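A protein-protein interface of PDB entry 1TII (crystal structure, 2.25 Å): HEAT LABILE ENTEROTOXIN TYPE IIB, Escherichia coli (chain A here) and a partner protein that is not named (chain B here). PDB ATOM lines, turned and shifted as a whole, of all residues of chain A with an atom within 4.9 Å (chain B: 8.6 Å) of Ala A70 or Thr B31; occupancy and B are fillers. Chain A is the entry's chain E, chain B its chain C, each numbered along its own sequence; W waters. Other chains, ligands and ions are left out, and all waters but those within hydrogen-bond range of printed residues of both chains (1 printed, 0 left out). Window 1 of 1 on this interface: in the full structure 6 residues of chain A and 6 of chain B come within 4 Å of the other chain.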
ATOM      1  N   LYS A  66       6.439  31.157 -17.713  1.00  0.00           N
ATOM      2  CA  LYS A  66       4.999  31.057 -17.957  1.00  0.00           C
ATOM      3  C   LYS A  66       4.710  30.655 -19.420  1.00  0.00           C
ATOM      4  O   LYS A  66       3.833  29.817 -19.701  1.00  0.00           O
ATOM      5  CB  LYS A  66       4.312  32.386 -17.688  1.00  0.00           C
ATOM      6  CG  LYS A  66       4.262  32.785 -16.246  1.00  0.00           C
ATOM      7  CD  LYS A  66       3.209  33.860 -16.044  1.00  0.00           C
ATOM      8  CE  LYS A  66       3.430  34.610 -14.745  1.00  0.00           C
ATOM      9  NZ  LYS A  66       2.382  35.646 -14.541  1.00  0.00           N
ATOM     10  N   ILE A  67       5.442  31.271 -20.349  1.00  0.00           N
ATOM     11  CA  ILE A  67       5.287  30.994 -21.785  1.00  0.00           C
ATOM     12  C   ILE A  67       5.606  29.526 -22.089  1.00  0.00           C
ATOM     13  O   ILE A  67       4.845  28.844 -22.769  1.00  0.00           O
ATOM     14  CB  ILE A  67       6.198  31.951 -22.654  1.00  0.00           C
ATOM     15  CG1 ILE A  67       5.669  33.392 -22.606  1.00  0.00           C
ATOM     16  CG2 ILE A  67       6.310  31.435 -24.076  1.00  0.00           C
ATOM     17  CD1 ILE A  67       6.733  34.451 -22.834  1.00  0.00           C
ATOM     18  N   ALA A  68       6.720  29.031 -21.562  1.00  0.00           N
ATOM     19  CA  ALA A  68       7.113  27.645 -21.774  1.00  0.00           C
ATOM     20  C   ALA A  68       6.035  26.689 -21.293  1.00  0.00           C
ATOM     21  O   ALA A  68       5.719  25.716 -21.976  1.00  0.00           O
ATOM     22  CB  ALA A  68       8.416  27.361 -21.062  1.00  0.00           C
ATOM     23  N   MET A  69       5.458  26.979 -20.128  1.00  0.00           N
ATOM     24  CA  MET A  69       4.414  26.141 -19.553  1.00  0.00           C
ATOM     25  C   MET A  69       3.129  26.237 -20.368  1.00  0.00           C
ATOM     26  O   MET A  69       2.450  25.233 -20.601  1.00  0.00           O
ATOM     27  CB  MET A  69       4.156  26.523 -18.093  1.00  0.00           C
ATOM     28  CG  MET A  69       2.994  25.768 -17.440  1.00  0.00           C
ATOM     29  SD  MET A  69       3.474  24.497 -16.258  1.00  0.00           S
ATOM     30  CE  MET A  69       3.912  25.547 -14.919  1.00  0.00           C
ATOM     31  N   ALA A  70       2.778  27.448 -20.783  1.00  0.00           N
ATOM     32  CA  ALA A  70       1.589  27.663 -21.609  1.00  0.00           C
ATOM     33  C   ALA A  70       1.707  26.842 -22.888  1.00  0.00           C
ATOM     34  O   ALA A  70       0.743  26.225 -23.316  1.00  0.00           O
ATOM     35  CB  ALA A  70       1.456  29.134 -21.953  1.00  0.00           C
ATOM     36  N   ALA A  71       2.916  26.786 -23.445  1.00  0.00           N
ATOM     37  CA  ALA A  71       3.188  26.046 -24.674  1.00  0.00           C
ATOM     38  C   ALA A  71       3.022  24.559 -24.490  1.00  0.00           C
ATOM     39  O   ALA A  71       2.389  23.901 -25.306  1.00  0.00           O
ATOM     40  CB  ALA A  71       4.593  26.353 -25.190  1.00  0.00           C
ATOM     41  N   VAL A  72       3.577  24.022 -23.409  1.00  0.00           N
ATOM     42  CA  VAL A  72       3.465  22.591 -23.152  1.00  0.00           C
ATOM     43  C   VAL A  72       2.026  22.181 -22.854  1.00  0.00           C
ATOM     44  O   VAL A  72       1.622  21.064 -23.200  1.00  0.00           O
ATOM     45  CB  VAL A  72       4.399  22.136 -21.990  1.00  0.00           C
ATOM     46  CG1 VAL A  72       4.197  20.633 -21.684  1.00  0.00           C
ATOM     47  CG2 VAL A  72       5.843  22.382 -22.373  1.00  0.00           C
ATOM     48  N   LEU A  73       1.258  23.074 -22.221  1.00  0.00           N
ATOM     49  CA  LEU A  73      -0.134  22.781 -21.870  1.00  0.00           C
ATOM     50  C   LEU A  73      -1.136  22.933 -23.014  1.00  0.00           C
ATOM     51  O   LEU A  73      -2.101  22.153 -23.114  1.00  0.00           O
ATOM     52  CB  LEU A  73      -0.609  23.649 -20.683  1.00  0.00           C
ATOM     53  CG  LEU A  73      -0.050  23.444 -19.258  1.00  0.00           C
ATOM     54  CD1 LEU A  73      -0.688  24.449 -18.314  1.00  0.00           C
ATOM     55  CD2 LEU A  73      -0.311  22.025 -18.778  1.00  0.00           C
ATOM     56  N   SER A  74      -0.927  23.950 -23.851  1.00  0.00           N
ATOM     57  CA  SER A  74      -1.832  24.250 -24.952  1.00  0.00           C
ATOM     58  C   SER A  74      -1.481  23.642 -26.292  1.00  0.00           C
ATOM     59  O   SER A  74      -2.352  23.278 -27.051  1.00  0.00           O
ATOM     60  CB  SER A  74      -1.955  25.761 -25.103  1.00  0.00           C
ATOM     61  OG  SER A  74      -0.721  26.300 -25.519  1.00  0.00           O
ATOM     62  N   GLY A  75      -0.199  23.496 -26.565  1.00  0.00           N
ATOM     63  CA  GLY A  75       0.208  22.982 -27.856  1.00  0.00           C
ATOM     64  C   GLY A  75       0.579  24.167 -28.753  1.00  0.00           C
ATOM     65  O   GLY A  75       0.950  23.991 -29.915  1.00  0.00           O
ATOM     66  N   LEU A  96       5.544  33.495 -27.922  1.00  0.00           N
ATOM     67  CA  LEU A  96       4.427  32.571 -27.910  1.00  0.00           C
ATOM     68  C   LEU A  96       3.506  33.082 -28.999  1.00  0.00           C
ATOM     69  O   LEU A  96       3.216  34.285 -29.038  1.00  0.00           O
ATOM     70  CB  LEU A  96       3.724  32.651 -26.557  1.00  0.00           C
ATOM     71  CG  LEU A  96       2.515  31.749 -26.349  1.00  0.00           C
ATOM     72  CD1 LEU A  96       2.960  30.310 -26.392  1.00  0.00           C
ATOM     73  CD2 LEU A  96       1.880  32.076 -25.009  1.00  0.00           C
ATOM     74  N   LYS B  24      -8.777  23.469 -30.187  1.00  0.00           N
ATOM     75  CA  LYS B  24      -7.716  24.384 -29.744  1.00  0.00           C
ATOM     76  C   LYS B  24      -8.278  25.381 -28.754  1.00  0.00           C
ATOM     77  O   LYS B  24      -7.619  25.753 -27.799  1.00  0.00           O
ATOM     78  CB  LYS B  24      -7.107  25.184 -30.895  1.00  0.00           C
ATOM     79  CG  LYS B  24      -6.330  24.405 -31.919  1.00  0.00           C
ATOM     80  CD  LYS B  24      -5.482  25.377 -32.735  1.00  0.00           C
ATOM     81  CE  LYS B  24      -5.058  24.800 -34.083  1.00  0.00           C
ATOM     82  NZ  LYS B  24      -6.079  25.000 -35.174  1.00  0.00           N
ATOM     83  N   TYR B  25      -9.481  25.859 -29.022  1.00  0.00           N
ATOM     84  CA  TYR B  25     -10.143  26.818 -28.150  1.00  0.00           C
ATOM     85  C   TYR B  25     -10.278  26.282 -26.709  1.00  0.00           C
ATOM     86  O   TYR B  25     -10.042  26.985 -25.730  1.00  0.00           O
ATOM     87  CB  TYR B  25     -11.530  27.121 -28.709  1.00  0.00           C
ATOM     88  CG  TYR B  25     -12.358  27.989 -27.800  1.00  0.00           C
ATOM     89  CD1 TYR B  25     -11.980  29.303 -27.543  1.00  0.00           C
ATOM     90  CD2 TYR B  25     -13.502  27.491 -27.171  1.00  0.00           C
ATOM     91  CE1 TYR B  25     -12.712  30.114 -26.680  1.00  0.00           C
ATOM     92  CE2 TYR B  25     -14.248  28.294 -26.306  1.00  0.00           C
ATOM     93  CZ  TYR B  25     -13.840  29.609 -26.070  1.00  0.00           C
ATOM     94  OH  TYR B  25     -14.562  30.437 -25.241  1.00  0.00           O
ATOM     95  N   ILE B  26     -10.739  25.045 -26.593  1.00  0.00           N
ATOM     96  CA  ILE B  26     -10.896  24.409 -25.295  1.00  0.00           C
ATOM     97  C   ILE B  26      -9.517  24.268 -24.588  1.00  0.00           C
ATOM     98  O   ILE B  26      -9.378  24.644 -23.416  1.00  0.00           O
ATOM     99  CB  ILE B  26     -11.633  23.033 -25.450  1.00  0.00           C
ATOM    100  CG1 ILE B  26     -13.112  23.248 -25.748  1.00  0.00           C
ATOM    101  CG2 ILE B  26     -11.524  22.213 -24.198  1.00  0.00           C
ATOM    102  CD1 ILE B  26     -13.800  24.178 -24.779  1.00  0.00           C
ATOM    103  N   LYS B  27      -8.498  23.807 -25.320  1.00  0.00           N
ATOM    104  CA  LYS B  27      -7.151  23.628 -24.768  1.00  0.00           C
ATOM    105  C   LYS B  27      -6.545  24.896 -24.259  1.00  0.00           C
ATOM    106  O   LYS B  27      -5.827  24.897 -23.260  1.00  0.00           O
ATOM    107  CB  LYS B  27      -6.181  23.053 -25.796  1.00  0.00           C
ATOM    108  CG  LYS B  27      -6.225  21.564 -25.931  1.00  0.00           C
ATOM    109  CD  LYS B  27      -4.877  20.914 -25.605  1.00  0.00           C
ATOM    110  CE  LYS B  27      -4.007  20.745 -26.856  1.00  0.00           C
ATOM    111  NZ  LYS B  27      -2.752  19.940 -26.640  1.00  0.00           N
ATOM    112  N   ARG B  28      -6.780  25.978 -24.979  1.00  0.00           N
ATOM    113  CA  ARG B  28      -6.218  27.248 -24.586  1.00  0.00           C
ATOM    114  C   ARG B  28      -6.977  27.845 -23.436  1.00  0.00           C
ATOM    115  O   ARG B  28      -6.376  28.496 -22.593  1.00  0.00           O
ATOM    116  CB  ARG B  28      -6.146  28.198 -25.784  1.00  0.00           C
ATOM    117  CG  ARG B  28      -5.222  27.675 -26.846  1.00  0.00           C
ATOM    118  CD  ARG B  28      -5.108  28.573 -28.027  1.00  0.00           C
ATOM    119  NE  ARG B  28      -4.311  27.900 -29.046  1.00  0.00           N
ATOM    120  CZ  ARG B  28      -3.929  28.449 -30.201  1.00  0.00           C
ATOM    121  NH1 ARG B  28      -4.275  29.704 -30.498  1.00  0.00           N
ATOM    122  NH2 ARG B  28      -3.186  27.738 -31.052  1.00  0.00           N
ATOM    123  N   LYS B  29      -8.286  27.629 -23.388  1.00  0.00           N
ATOM    124  CA  LYS B  29      -9.075  28.141 -22.271  1.00  0.00           C
ATOM    125  C   LYS B  29      -8.699  27.362 -20.984  1.00  0.00           C
ATOM    126  O   LYS B  29      -8.523  27.943 -19.908  1.00  0.00           O
ATOM    127  CB  LYS B  29     -10.567  28.014 -22.546  1.00  0.00           C
ATOM    128  CG  LYS B  29     -11.357  28.977 -21.694  1.00  0.00           C
ATOM    129  CD  LYS B  29     -12.822  28.788 -21.886  1.00  0.00           C
ATOM    130  CE  LYS B  29     -13.610  29.781 -21.085  1.00  0.00           C
ATOM    131  NZ  LYS B  29     -15.058  29.597 -21.408  1.00  0.00           N
ATOM    132  N   PHE B  30      -8.589  26.044 -21.101  1.00  0.00           N
ATOM    133  CA  PHE B  30      -8.184  25.223 -19.971  1.00  0.00           C
ATOM    134  C   PHE B  30      -6.806  25.697 -19.492  1.00  0.00           C
ATOM    135  O   PHE B  30      -6.627  25.990 -18.317  1.00  0.00           O
ATOM    136  CB  PHE B  30      -8.098  23.764 -20.377  1.00  0.00           C
ATOM    137  CG  PHE B  30      -7.382  22.921 -19.373  1.00  0.00           C
ATOM    138  CD1 PHE B  30      -8.038  22.476 -18.232  1.00  0.00           C
ATOM    139  CD2 PHE B  30      -6.027  22.632 -19.532  1.00  0.00           C
ATOM    140  CE1 PHE B  30      -7.364  21.766 -17.263  1.00  0.00           C
ATOM    141  CE2 PHE B  30      -5.347  21.927 -18.570  1.00  0.00           C
ATOM    142  CZ  PHE B  30      -6.022  21.493 -17.426  1.00  0.00           C
ATOM    143  N   THR B  31      -5.848  25.782 -20.416  1.00  0.00           N
ATOM    144  CA  THR B  31      -4.498  26.252 -20.114  1.00  0.00           C
ATOM    145  C   THR B  31      -4.525  27.574 -19.348  1.00  0.00           C
ATOM    146  O   THR B  31      -3.813  27.737 -18.355  1.00  0.00           O
ATOM    147  CB  THR B  31      -3.680  26.470 -21.401  1.00  0.00           C
ATOM    148  OG1 THR B  31      -3.441  25.215 -22.033  1.00  0.00           O
ATOM    149  CG2 THR B  31      -2.345  27.111 -21.101  1.00  0.00           C
ATOM    150  N   LEU B  32      -5.345  28.509 -19.810  1.00  0.00           N
ATOM    151  CA  LEU B  32      -5.463  29.823 -19.195  1.00  0.00           C
ATOM    152  C   LEU B  32      -5.982  29.764 -17.766  1.00  0.00           C
ATOM    153  O   LEU B  32      -5.515  30.501 -16.909  1.00  0.00           O
ATOM    154  CB  LEU B  32      -6.377  30.718 -20.047  1.00  0.00           C
ATOM    155  CG  LEU B  32      -6.805  32.089 -19.515  1.00  0.00           C
ATOM    156  CD1 LEU B  32      -5.596  32.999 -19.413  1.00  0.00           C
ATOM    157  CD2 LEU B  32      -7.865  32.701 -20.427  1.00  0.00           C
ATOM    158  N   MET B  33      -7.003  28.954 -17.521  1.00  0.00           N
ATOM    159  CA  MET B  33      -7.540  28.843 -16.170  1.00  0.00           C
ATOM    160  C   MET B  33      -6.504  28.165 -15.267  1.00  0.00           C
ATOM    161  O   MET B  33      -6.358  28.545 -14.117  1.00  0.00           O
ATOM    162  CB  MET B  33      -8.863  28.072 -16.162  1.00  0.00           C
ATOM    163  CG  MET B  33      -9.961  28.686 -17.023  1.00  0.00           C
ATOM    164  SD  MET B  33     -10.626  30.257 -16.415  1.00  0.00           S
ATOM    165  CE  MET B  33      -9.847  31.345 -17.480  1.00  0.00           C
ATOM    166  N   THR B  34      -5.743  27.222 -15.815  1.00  0.00           N
ATOM    167  CA  THR B  34      -4.701  26.524 -15.059  1.00  0.00           C
ATOM    168  C   THR B  34      -3.565  27.450 -14.644  1.00  0.00           C
ATOM    169  O   THR B  34      -3.142  27.427 -13.489  1.00  0.00           O
ATOM    170  CB  THR B  34      -4.117  25.363 -15.848  1.00  0.00           C
ATOM    171  OG1 THR B  34      -5.143  24.406 -16.098  1.00  0.00           O
ATOM    172  CG2 THR B  34      -2.985  24.704 -15.091  1.00  0.00           C
ATOM    173  N   LEU B  35      -3.074  28.276 -15.568  1.00  0.00           N
ATOM    174  CA  LEU B  35      -1.984  29.207 -15.248  1.00  0.00           C
ATOM    175  C   LEU B  35      -2.424  30.230 -14.233  1.00  0.00           C
ATOM    176  O   LEU B  35      -1.618  30.705 -13.447  1.00  0.00           O
ATOM    177  CB  LEU B  35      -1.438  29.940 -16.482  1.00  0.00           C
ATOM    178  CG  LEU B  35      -0.766  29.135 -17.584  1.00  0.00           C
ATOM    179  CD1 LEU B  35      -0.397  30.087 -18.690  1.00  0.00           C
ATOM    180  CD2 LEU B  35       0.442  28.411 -17.091  1.00  0.00           C
ATOM    181  N   LEU B  36      -3.690  30.603 -14.277  1.00  0.00           N
ATOM    182  CA  LEU B  36      -4.238  31.568 -13.331  1.00  0.00           C
ATOM    183  C   LEU B  36      -4.316  30.929 -11.932  1.00  0.00           C
ATOM    184  O   LEU B  36      -4.128  31.613 -10.935  1.00  0.00           O
ATOM    185  CB  LEU B  36      -5.641  31.995 -13.764  1.00  0.00           C
ATOM    186  CG  LEU B  36      -6.311  33.006 -12.833  1.00  0.00           C
ATOM    187  CD1 LEU B  36      -5.857  34.395 -13.215  1.00  0.00           C
ATOM    188  CD2 LEU B  36      -7.826  32.893 -12.889  1.00  0.00           C
ATOM    189  N   SER B  37      -4.653  29.638 -11.875  1.00  0.00           N
ATOM    190  CA  SER B  37      -4.758  28.900 -10.616  1.00  0.00           C
ATOM    191  C   SER B  37      -3.413  28.609  -9.933  1.00  0.00           C
ATOM    192  O   SER B  37      -3.258  28.847  -8.739  1.00  0.00           O
ATOM    193  CB  SER B  37      -5.496  27.583 -10.845  1.00  0.00           C
ATOM    194  OG  SER B  37      -6.832  27.827 -11.217  1.00  0.00           O
ATOM    195  N   ILE B  38      -2.438  28.144 -10.713  1.00  0.00           N
ATOM    196  CA  ILE B  38      -1.110  27.786 -10.206  1.00  0.00           C
ATOM    197  C   ILE B  38      -0.089  28.907 -10.023  1.00  0.00           C
ATOM    198  O   ILE B  38       0.983  28.679  -9.469  1.00  0.00           O
ATOM    199  CB  ILE B  38      -0.436  26.730 -11.108  1.00  0.00           C
ATOM    200  CG1 ILE B  38      -0.015  27.350 -12.444  1.00  0.00           C
ATOM    201  CG2 ILE B  38      -1.375  25.564 -11.328  1.00  0.00           C
ATOM    202  CD1 ILE B  38       0.652  26.382 -13.388  1.00  0.00           C
ATOM    203  N   ASN B  39      -0.393  30.115 -10.481  1.00  0.00           N
ATOM    204  CA  ASN B  39       0.581  31.188 -10.371  1.00  0.00           C
ATOM    205  C   ASN B  39       0.330  32.096  -9.207  1.00  0.00           C
ATOM    206  O   ASN B  39      -0.809  32.431  -8.890  1.00  0.00           O
ATOM    207  CB  ASN B  39       0.758  31.940 -11.705  1.00  0.00           C
ATOM    208  CG  ASN B  39       1.695  31.200 -12.679  1.00  0.00           C
ATOM    209  OD1 ASN B  39       2.916  31.279 -12.560  1.00  0.00           O
ATOM    210  ND2 ASN B  39       1.119  30.470 -13.627  1.00  0.00           N
HETATM  211  O   HOH W   1      -3.527  25.217 -28.821  1.00  0.00           O
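O of Ser A74 sits close to NZ of Lys B27, 3.4 Å away.
The backbone NH of Ser A74 lies within hydrogen-bond range of the side-chain hydroxyl of Thr B31, 3.4 Å away.
The backbone carbonyl oxygen (O) of Ala A70 sits at hydrogen-bond distance from the side-chain hydroxyl (OG) of Ser A74.
The backbone carbonyl oxygen (O) of Lys B27 is in hydrogen-bond range of the side-chain hydroxyl (OG1) of Thr B31 (2.7 Å).
O of Phe B30 sits at hydrogen-bond distance from OG1 of Thr B34, at 3.1 Å.
O of Leu B35 lies within hydrogen-bond range of ND2 of Asn B39 (2.8 Å).
Among the printed residues, merely in contact across the chains: Met A69 with Leu B35 (3.7 Å), Met A69 with Ile B38 (3.7 Å), Ala A70 with Thr B31 (3.9 Å), Ala A70 with Leu B35 (3.9 Å), Leu A73 with Lys B27 (3.9 Å), Leu A73 with Thr B31 (3.4 Å) and Leu A73 with Thr B34 (3.97 Å).
Ile A67 touches none of the printed residues of chain B.
Of the printed residues of chain B, Met A69 touches Leu B35 and Ile B38.
Of chain B, only Thr B31 (3.9 Å) and Leu B35 (3.9 Å) come within 4 Å of Ala A70.
Val A72 touches none of the printed residues of chain B.
Of the printed residues of chain B, Ser A74 touches Lys B27 (3.0 Å) and Thr B31 (3.4 Å).
Of the printed residues of chain A, Lys B27 touches Leu A73 (3.9 Å) and Ser A74 (3.0 Å).
Of chain A, only Ala A70 (3.9 Å), Leu A73 (3.4 Å) and Ser A74 (3.4 Å) come within 4 Å of Thr B31.
Of the printed residues of chain A, Leu B35 touches Met A69 and Ala A70.
Of the printed residues of chain A, Ile B38 touches Met A69.
The nearest printed residue of chain B that does not touch Met A69 is Thr B31 (5.2 Å).
Of the 16 printed residues of chain B, 5 touch a printed residue of chain A.
Along chain B the printed residues that touch a printed residue of chain A span positions 27 to 38.
Of the 11 printed residues of chain A, 4 touch a printed residue of chain B.
Among the printed residues, no Asp or Glu carboxylate lies within 4 Å of a Lys or Arg side-chain nitrogen of the other chain.
Water W1 bridges the guanidinium group (NE) of Arg B28 and the backbone carbonyl oxygen (O) of Ser A74.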
